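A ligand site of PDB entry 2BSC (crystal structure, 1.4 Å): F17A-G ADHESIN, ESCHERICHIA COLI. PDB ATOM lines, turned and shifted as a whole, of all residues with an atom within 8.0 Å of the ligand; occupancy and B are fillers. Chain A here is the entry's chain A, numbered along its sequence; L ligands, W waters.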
ATOM      1  N   GLN A  41       1.575   1.711  -0.107  1.00  0.00           N
ATOM      2  CA  GLN A  41       0.846   2.962  -0.089  1.00  0.00           C
ATOM      3  C   GLN A  41       0.802   3.557  -1.491  1.00  0.00           C
ATOM      4  O   GLN A  41       1.815   3.604  -2.186  1.00  0.00           O
ATOM      5  CB  GLN A  41       1.532   3.945   0.878  1.00  0.00           C
ATOM      6  CG  GLN A  41       0.825   5.275   1.030  1.00  0.00           C
ATOM      7  CD  GLN A  41       1.570   6.189   1.989  1.00  0.00           C
ATOM      8  OE1 GLN A  41       2.738   6.525   1.770  1.00  0.00           O
ATOM      9  NE2 GLN A  41       0.897   6.596   3.061  1.00  0.00           N
ATOM     10  N   ASN A  42      -0.376   4.000  -1.908  1.00  0.00           N
ATOM     11  CA  ASN A  42      -0.555   4.613  -3.214  1.00  0.00           C
ATOM     12  C   ASN A  42      -1.683   5.634  -3.122  1.00  0.00           C
ATOM     13  O   ASN A  42      -2.840   5.263  -2.969  1.00  0.00           O
ATOM     14  CB  ASN A  42      -0.884   3.561  -4.270  1.00  0.00           C
ATOM     15  CG  ASN A  42      -0.779   4.093  -5.685  1.00  0.00           C
ATOM     16  OD1 ASN A  42      -0.738   5.313  -5.901  1.00  0.00           O
ATOM     17  ND2 ASN A  42      -0.722   3.195  -6.665  1.00  0.00           N
ATOM     18  N   ALA A  43      -1.344   6.908  -3.206  1.00  0.00           N
ATOM     19  CA  ALA A  43      -2.356   7.949  -3.123  1.00  0.00           C
ATOM     20  C   ALA A  43      -3.262   8.018  -4.344  1.00  0.00           C
ATOM     21  O   ALA A  43      -4.331   8.607  -4.295  1.00  0.00           O
ATOM     22  CB  ALA A  43      -1.691   9.284  -2.920  1.00  0.00           C
ATOM     23  N   ASN A  44      -2.843   7.370  -5.433  1.00  0.00           N
ATOM     24  CA  ASN A  44      -3.571   7.452  -6.688  1.00  0.00           C
ATOM     25  C   ASN A  44      -3.944   6.110  -7.308  1.00  0.00           C
ATOM     26  O   ASN A  44      -3.236   5.594  -8.170  1.00  0.00           O
ATOM     27  CB  ASN A  44      -2.708   8.261  -7.660  1.00  0.00           C
ATOM     28  CG  ASN A  44      -1.984   9.404  -6.950  1.00  0.00           C
ATOM     29  OD1 ASN A  44      -2.612  10.336  -6.463  1.00  0.00           O
ATOM     30  ND2 ASN A  44      -0.660   9.308  -6.870  1.00  0.00           N
ATOM     31  N   VAL A  45      -5.061   5.547  -6.863  1.00  0.00           N
ATOM     32  CA  VAL A  45      -5.505   4.268  -7.374  1.00  0.00           C
ATOM     33  C   VAL A  45      -6.714   4.491  -8.291  1.00  0.00           C
ATOM     34  O   VAL A  45      -6.927   3.741  -9.249  1.00  0.00           O
ATOM     35  CB  VAL A  45      -5.850   3.309  -6.215  1.00  0.00           C
ATOM     36  CG1 VAL A  45      -6.368   1.978  -6.743  1.00  0.00           C
ATOM     37  CG2 VAL A  45      -4.597   3.073  -5.379  1.00  0.00           C
ATOM     38  N   TRP A  46      -7.485   5.541  -8.003  1.00  0.00           N
ATOM     39  CA  TRP A  46      -8.648   5.920  -8.797  1.00  0.00           C
ATOM     40  C   TRP A  46      -8.621   7.435  -8.954  1.00  0.00           C
ATOM     41  O   TRP A  46      -8.182   8.152  -8.052  1.00  0.00           O
ATOM     42  CB  TRP A  46      -9.972   5.544  -8.117  1.00  0.00           C
ATOM     43  CG  TRP A  46     -10.240   4.083  -8.077  1.00  0.00           C
ATOM     44  CD1 TRP A  46     -10.731   3.305  -9.072  1.00  0.00           C
ATOM     45  CD2 TRP A  46      -9.980   3.214  -6.973  1.00  0.00           C
ATOM     46  NE1 TRP A  46     -10.800   1.994  -8.676  1.00  0.00           N
ATOM     47  CE2 TRP A  46     -10.335   1.903  -7.382  1.00  0.00           C
ATOM     48  CE3 TRP A  46      -9.471   3.402  -5.683  1.00  0.00           C
ATOM     49  CZ2 TRP A  46     -10.205   0.795  -6.552  1.00  0.00           C
ATOM     50  CZ3 TRP A  46      -9.339   2.303  -4.853  1.00  0.00           C
ATOM     51  CH2 TRP A  46      -9.711   1.016  -5.291  1.00  0.00           C
ATOM     52  N   ILE A  48     -10.989  10.626  -9.388  1.00  0.00           N
ATOM     53  CA  ILE A  48     -12.395  10.958  -9.180  1.00  0.00           C
ATOM     54  C   ILE A  48     -12.663  12.439  -9.429  1.00  0.00           C
ATOM     55  O   ILE A  48     -11.773  13.275  -9.267  1.00  0.00           O
ATOM     56  CB  ILE A  48     -12.875  10.530  -7.759  1.00  0.00           C
ATOM     57  CG1 ILE A  48     -11.935  11.071  -6.673  1.00  0.00           C
ATOM     58  CG2 ILE A  48     -12.882   9.018  -7.660  1.00  0.00           C
ATOM     59  CD1 ILE A  48     -11.931  12.547  -6.519  1.00  0.00           C
ATOM     60  N   VAL A  54     -16.678   8.405  -2.567  1.00  0.00           N
ATOM     61  CA  VAL A  54     -16.106   7.075  -2.465  1.00  0.00           C
ATOM     62  C   VAL A  54     -15.421   6.747  -1.145  1.00  0.00           C
ATOM     63  O   VAL A  54     -14.799   7.616  -0.520  1.00  0.00           O
ATOM     64  CB  VAL A  54     -15.115   6.838  -3.639  1.00  0.00           C
ATOM     65  CG1 VAL A  54     -13.925   7.777  -3.516  1.00  0.00           C
ATOM     66  CG2 VAL A  54     -14.664   5.394  -3.665  1.00  0.00           C
ATOM     67  N   LEU A  56     -13.762   2.919   1.084  1.00  0.00           N
ATOM     68  CA  LEU A  56     -13.033   1.683   0.803  1.00  0.00           C
ATOM     69  C   LEU A  56     -13.439   0.528   1.713  1.00  0.00           C
ATOM     70  O   LEU A  56     -13.706   0.731   2.901  1.00  0.00           O
ATOM     71  CB  LEU A  56     -11.523   1.880   0.959  1.00  0.00           C
ATOM     72  CG  LEU A  56     -10.760   2.960   0.191  1.00  0.00           C
ATOM     73  CD1 LEU A  56      -9.362   3.104   0.791  1.00  0.00           C
ATOM     74  CD2 LEU A  56     -10.690   2.618  -1.312  1.00  0.00           C
ATOM     75  N   GLY A  87      -6.767   0.766   4.760  1.00  0.00           N
ATOM     76  CA  GLY A  87      -7.492   2.017   4.832  1.00  0.00           C
ATOM     77  C   GLY A  87      -7.093   3.015   3.778  1.00  0.00           C
ATOM     78  O   GLY A  87      -6.496   2.662   2.753  1.00  0.00           O
ATOM     79  N   ASP A  88      -7.429   4.276   4.034  1.00  0.00           N
ATOM     80  CA  ASP A  88      -7.096   5.380   3.140  1.00  0.00           C
ATOM     81  C   ASP A  88      -5.580   5.517   3.021  1.00  0.00           C
ATOM     82  O   ASP A  88      -4.815   4.895   3.766  1.00  0.00           O
ATOM     83  CB  ASP A  88      -7.746   6.651   3.680  1.00  0.00           C
ATOM     84  CG  ASP A  88      -7.774   7.779   2.679  1.00  0.00           C
ATOM     85  OD1 ASP A  88      -7.758   7.489   1.458  1.00  0.00           O
ATOM     86  OD2 ASP A  88      -7.841   8.949   3.106  1.00  0.00           O
ATOM     87  N   THR A  89      -5.133   6.338   2.073  1.00  0.00           N
ATOM     88  CA  THR A  89      -3.721   6.553   1.801  1.00  0.00           C
ATOM     89  C   THR A  89      -2.752   6.672   2.980  1.00  0.00           C
ATOM     90  O   THR A  89      -1.794   5.890   3.086  1.00  0.00           O
ATOM     91  CB  THR A  89      -3.529   7.799   0.925  1.00  0.00           C
ATOM     92  OG1 THR A  89      -4.374   7.698  -0.219  1.00  0.00           O
ATOM     93  CG2 THR A  89      -2.074   7.936   0.485  1.00  0.00           C
ATOM     94  N   LYS A  90      -2.980   7.647   3.850  1.00  0.00           N
ATOM     95  CA  LYS A  90      -2.084   7.848   4.989  1.00  0.00           C
ATOM     96  C   LYS A  90      -2.150   6.715   6.005  1.00  0.00           C
ATOM     97  O   LYS A  90      -3.212   6.345   6.478  1.00  0.00           O
ATOM     98  CB  LYS A  90      -2.354   9.214   5.640  1.00  0.00           C
ATOM     99  CG  LYS A  90      -2.015  10.355   4.691  1.00  0.00           C
ATOM    100  CD  LYS A  90      -2.196  11.726   5.305  1.00  0.00           C
ATOM    101  CE  LYS A  90      -1.891  12.814   4.279  1.00  0.00           C
ATOM    102  NZ  LYS A  90      -2.141  14.181   4.800  1.00  0.00           N
ATOM    103  N   ARG A  93      -4.375   6.318   9.063  1.00  0.00           N
ATOM    104  CA  ARG A  93      -5.811   6.171   8.819  1.00  0.00           C
ATOM    105  C   ARG A  93      -6.191   4.696   8.691  1.00  0.00           C
ATOM    106  O   ARG A  93      -7.345   4.358   8.454  1.00  0.00           O
ATOM    107  CB  ARG A  93      -6.213   6.888   7.521  1.00  0.00           C
ATOM    108  CG  ARG A  93      -5.766   8.340   7.419  1.00  0.00           C
ATOM    109  CD  ARG A  93      -6.506   9.261   8.387  1.00  0.00           C
ATOM    110  NE  ARG A  93      -5.758  10.502   8.624  1.00  0.00           N
ATOM    111  CZ  ARG A  93      -5.540  11.439   7.713  1.00  0.00           C
ATOM    112  NH1 ARG A  93      -4.841  12.518   8.036  1.00  0.00           N
ATOM    113  NH2 ARG A  93      -6.043  11.314   6.493  1.00  0.00           N
ATOM    114  N   PHE A 106     -12.468   2.628   5.264  1.00  0.00           N
ATOM    115  CA  PHE A 106     -12.403   4.079   5.031  1.00  0.00           C
ATOM    116  C   PHE A 106     -13.839   4.534   4.757  1.00  0.00           C
ATOM    117  O   PHE A 106     -14.422   4.186   3.734  1.00  0.00           O
ATOM    118  CB  PHE A 106     -11.509   4.418   3.833  1.00  0.00           C
ATOM    119  CG  PHE A 106     -11.496   5.902   3.487  1.00  0.00           C
ATOM    120  CD1 PHE A 106     -11.403   6.863   4.494  1.00  0.00           C
ATOM    121  CD2 PHE A 106     -11.556   6.326   2.161  1.00  0.00           C
ATOM    122  CE1 PHE A 106     -11.391   8.234   4.191  1.00  0.00           C
ATOM    123  CE2 PHE A 106     -11.544   7.686   1.848  1.00  0.00           C
ATOM    124  CZ  PHE A 106     -11.466   8.641   2.862  1.00  0.00           C
ATOM    125  N   GLY A 108     -15.017   7.238   3.775  1.00  0.00           N
ATOM    126  CA  GLY A 108     -15.176   7.919   2.499  1.00  0.00           C
ATOM    127  C   GLY A 108     -15.269   9.439   2.485  1.00  0.00           C
ATOM    128  O   GLY A 108     -15.357  10.088   3.523  1.00  0.00           O
ATOM    129  N   TRP A 109     -15.225   9.983   1.271  1.00  0.00           N
ATOM    130  CA  TRP A 109     -15.324  11.428   1.075  1.00  0.00           C
ATOM    131  C   TRP A 109     -15.872  11.685  -0.324  1.00  0.00           C
ATOM    132  O   TRP A 109     -15.943  10.774  -1.151  1.00  0.00           O
ATOM    133  CB  TRP A 109     -13.961  12.112   1.222  1.00  0.00           C
ATOM    134  CG  TRP A 109     -13.009  11.886   0.077  1.00  0.00           C
ATOM    135  CD1 TRP A 109     -12.525  10.693  -0.383  1.00  0.00           C
ATOM    136  CD2 TRP A 109     -12.418  12.898  -0.754  1.00  0.00           C
ATOM    137  NE1 TRP A 109     -11.679  10.893  -1.445  1.00  0.00           N
ATOM    138  CE2 TRP A 109     -11.583  12.241  -1.691  1.00  0.00           C
ATOM    139  CE3 TRP A 109     -12.504  14.291  -0.795  1.00  0.00           C
ATOM    140  CZ2 TRP A 109     -10.852  12.931  -2.658  1.00  0.00           C
ATOM    141  CZ3 TRP A 109     -11.770  14.980  -1.772  1.00  0.00           C
ATOM    142  CH2 TRP A 109     -10.961  14.300  -2.682  1.00  0.00           C
ATOM    143  N   CYS A 110     -16.283  12.925  -0.568  1.00  0.00           N
ATOM    144  CA  CYS A 110     -16.791  13.308  -1.884  1.00  0.00           C
ATOM    145  C   CYS A 110     -15.954  14.456  -2.417  1.00  0.00           C
ATOM    146  O   CYS A 110     -15.711  15.441  -1.725  1.00  0.00           O
ATOM    147  CB  CYS A 110     -18.230  13.782  -1.794  1.00  0.00           C
ATOM    148  SG  CYS A 110     -19.422  12.656  -1.011  1.00  0.00           S
ATOM    149  N   VAL A 111     -15.509  14.316  -3.666  1.00  0.00           N
ATOM    150  CA  VAL A 111     -14.723  15.361  -4.297  1.00  0.00           C
ATOM    151  C   VAL A 111     -15.690  16.471  -4.742  1.00  0.00           C
ATOM    152  O   VAL A 111     -16.882  16.227  -4.947  1.00  0.00           O
ATOM    153  CB  VAL A 111     -13.936  14.795  -5.518  1.00  0.00           C
ATOM    154  CG1 VAL A 111     -14.897  14.384  -6.633  1.00  0.00           C
ATOM    155  CG2 VAL A 111     -12.928  15.813  -6.020  1.00  0.00           C
ATOM    156  N   ALA A 116     -11.472  17.869  -9.437  1.00  0.00           N
ATOM    157  CA  ALA A 116     -10.962  16.520  -9.602  1.00  0.00           C
ATOM    158  C   ALA A 116      -9.892  16.234  -8.573  1.00  0.00           C
ATOM    159  O   ALA A 116      -9.232  17.152  -8.057  1.00  0.00           O
ATOM    160  CB  ALA A 116     -10.379  16.360 -10.996  1.00  0.00           C
ATOM    161  N   SER A 117      -9.717  14.957  -8.267  1.00  0.00           N
ATOM    162  CA  SER A 117      -8.710  14.511  -7.313  1.00  0.00           C
ATOM    163  C   SER A 117      -8.504  13.006  -7.540  1.00  0.00           C
ATOM    164  O   SER A 117      -8.889  12.458  -8.569  1.00  0.00           O
ATOM    165  CB  SER A 117      -9.154  14.789  -5.880  1.00  0.00           C
ATOM    166  OG  SER A 117      -8.097  14.599  -4.969  1.00  0.00           O
ATOM    167  N   THR A 118      -7.884  12.346  -6.572  1.00  0.00           N
ATOM    168  CA  THR A 118      -7.662  10.912  -6.686  1.00  0.00           C
ATOM    169  C   THR A 118      -8.026  10.273  -5.367  1.00  0.00           C
ATOM    170  O   THR A 118      -8.164  10.956  -4.346  1.00  0.00           O
ATOM    171  CB  THR A 118      -6.171  10.596  -6.975  1.00  0.00           C
ATOM    172  OG1 THR A 118      -5.350  11.138  -5.925  1.00  0.00           O
ATOM    173  CG2 THR A 118      -5.728  11.192  -8.309  1.00  0.00           C
ATOM    174  N   GLN A 119      -8.222   8.957  -5.394  1.00  0.00           N
ATOM    175  CA  GLN A 119      -8.527   8.195  -4.192  1.00  0.00           C
ATOM    176  C   GLN A 119      -7.428   7.166  -4.062  1.00  0.00           C
ATOM    177  O   GLN A 119      -7.150   6.436  -5.016  1.00  0.00           O
ATOM    178  CB  GLN A 119      -9.889   7.501  -4.317  1.00  0.00           C
ATOM    179  CG  GLN A 119     -10.207   6.534  -3.181  1.00  0.00           C
ATOM    180  CD  GLN A 119     -10.226   7.191  -1.810  1.00  0.00           C
ATOM    181  OE1 GLN A 119     -10.857   8.222  -1.605  1.00  0.00           O
ATOM    182  NE2 GLN A 119      -9.527   6.582  -0.845  1.00  0.00           N
ATOM    183  N   GLY A 120      -6.808   7.102  -2.893  1.00  0.00           N
ATOM    184  CA  GLY A 120      -5.727   6.164  -2.662  1.00  0.00           C
ATOM    185  C   GLY A 120      -6.051   5.134  -1.595  1.00  0.00           C
ATOM    186  O   GLY A 120      -7.205   4.954  -1.220  1.00  0.00           O
ATOM    187  N   LEU A 121      -5.011   4.462  -1.111  1.00  0.00           N
ATOM    188  CA  LEU A 121      -5.189   3.443  -0.086  1.00  0.00           C
ATOM    189  C   LEU A 121      -3.845   3.030   0.481  1.00  0.00           C
ATOM    190  O   LEU A 121      -2.796   3.392  -0.057  1.00  0.00           O
ATOM    191  CB  LEU A 121      -5.882   2.211  -0.695  1.00  0.00           C
ATOM    192  CG  LEU A 121      -5.265   1.608  -1.961  1.00  0.00           C
ATOM    193  CD1 LEU A 121      -3.954   0.887  -1.655  1.00  0.00           C
ATOM    194  CD2 LEU A 121      -6.262   0.626  -2.558  1.00  0.00           C
ATOM    195  N   SER A 122      -3.888   2.287   1.590  1.00  0.00           N
ATOM    196  CA  SER A 122      -2.678   1.799   2.210  1.00  0.00           C
ATOM    197  C   SER A 122      -2.964   0.481   2.909  1.00  0.00           C
ATOM    198  O   SER A 122      -4.086   0.231   3.363  1.00  0.00           O
ATOM    199  CB  SER A 122      -2.131   2.810   3.227  1.00  0.00           C
ATOM    200  OG  SER A 122      -2.977   2.923   4.352  1.00  0.00           O
HETATM  201  C1  LIG L   1      -6.812  13.022  -1.790  1.00  0.00           C
HETATM  202  C2  LIG L   1      -5.633  12.050  -1.863  1.00  0.00           C
HETATM  203  C3  LIG L   1      -6.064  10.633  -1.917  1.00  0.00           C
HETATM  204  C4  LIG L   1      -6.904  10.321  -0.695  1.00  0.00           C
HETATM  205  C5  LIG L   1      -8.072  11.176  -0.587  1.00  0.00           C
HETATM  206  C6  LIG L   1      -9.059  11.007   0.536  1.00  0.00           C
HETATM  207  C7  LIG L   1      -3.703  12.810  -2.961  1.00  0.00           C
HETATM  208  C8  LIG L   1      -2.878  13.102  -4.321  1.00  0.00           C
HETATM  209  N1  LIG L   1      -4.826  12.403  -3.046  1.00  0.00           N
HETATM  210  O1  LIG L   1      -6.436  14.457  -1.681  1.00  0.00           O
HETATM  211  O2  LIG L   1      -4.896   9.747  -1.949  1.00  0.00           O
HETATM  212  O3  LIG L   1      -7.326   8.879  -0.765  1.00  0.00           O
HETATM  213  O4  LIG L   1      -7.612  12.606  -0.578  1.00  0.00           O
HETATM  214  O5  LIG L   1      -8.287  11.318   1.784  1.00  0.00           O
HETATM  215  O6  LIG L   1      -2.880  13.059  -1.995  1.00  0.00           O
HETATM  216  O   HOH W   1      -2.695  11.949   0.473  1.00  0.00           O
HETATM  217  O   HOH W   2     -10.357  13.382   3.549  1.00  0.00           O
HETATM  218  O   HOH W   3      -5.555  14.604   1.133  1.00  0.00           O
HETATM  219  O   HOH W   4      -0.165  14.447  -2.333  1.00  0.00           O
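The side-chain hydroxyl (OG1) of Thr 89 is in hydrogen-bond range of an oxygen (O2) of the ligand, 2.7 Å away.
The backbone carbonyl oxygen of Ala 43 is in hydrogen-bond range of an oxygen (O2) of the ligand (2.7 Å).
The side-chain amide nitrogen (NE2) of Gln 119 lies within hydrogen-bond range of an oxygen (O3) of the ligand, 3.2 Å away.
OD1 of Asp 88 is in hydrogen-bond range of O3 of the ligand, 2.7 Å away.
The side-chain hydroxyl (OG1) of Thr 118 sits at hydrogen-bond distance from a nitrogen (N1) of the ligand (3.2 Å).
O3 of the ligand lies within hydrogen-bond range of N of Gly 120.
The side-chain hydroxyl (OG1) of Thr 118 lies within hydrogen-bond range of the backbone carbonyl oxygen (O) of Ala 43.
The backbone NH of Asn 44 lies within hydrogen-bond range of the side-chain amide oxygen of Asn 42 (3.0 Å).
The backbone NH (N) of Gln 119 lies within hydrogen-bond range of the backbone carbonyl oxygen (O) of Trp 46 (2.8 Å).
The backbone carbonyl oxygen of Trp 109 is in hydrogen-bond range of the backbone NH of Val 54, at 2.9 Å.
O of Ala 43 is in hydrogen-bond range of N of Gly 120 (3.2 Å).
N of Ser 117 lies within hydrogen-bond range of O of Ile 48.
The backbone carbonyl oxygen of Asp 88 sits at hydrogen-bond distance from the side-chain hydroxyl of Ser 122 (2.8 Å).
The backbone carbonyl oxygen (O) of Gln 119 sits at hydrogen-bond distance from the backbone NH (N) of Val 45 (2.9 Å).
Merely in contact with the ligand: Asn 44, Trp 109 and Ser 117.
Hydrophobic or aromatic side chains that line the ligand: Ala 43 and Trp 109.
The nearest printed residue that does not touch the ligand is Phe 106 (4.1 Å).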
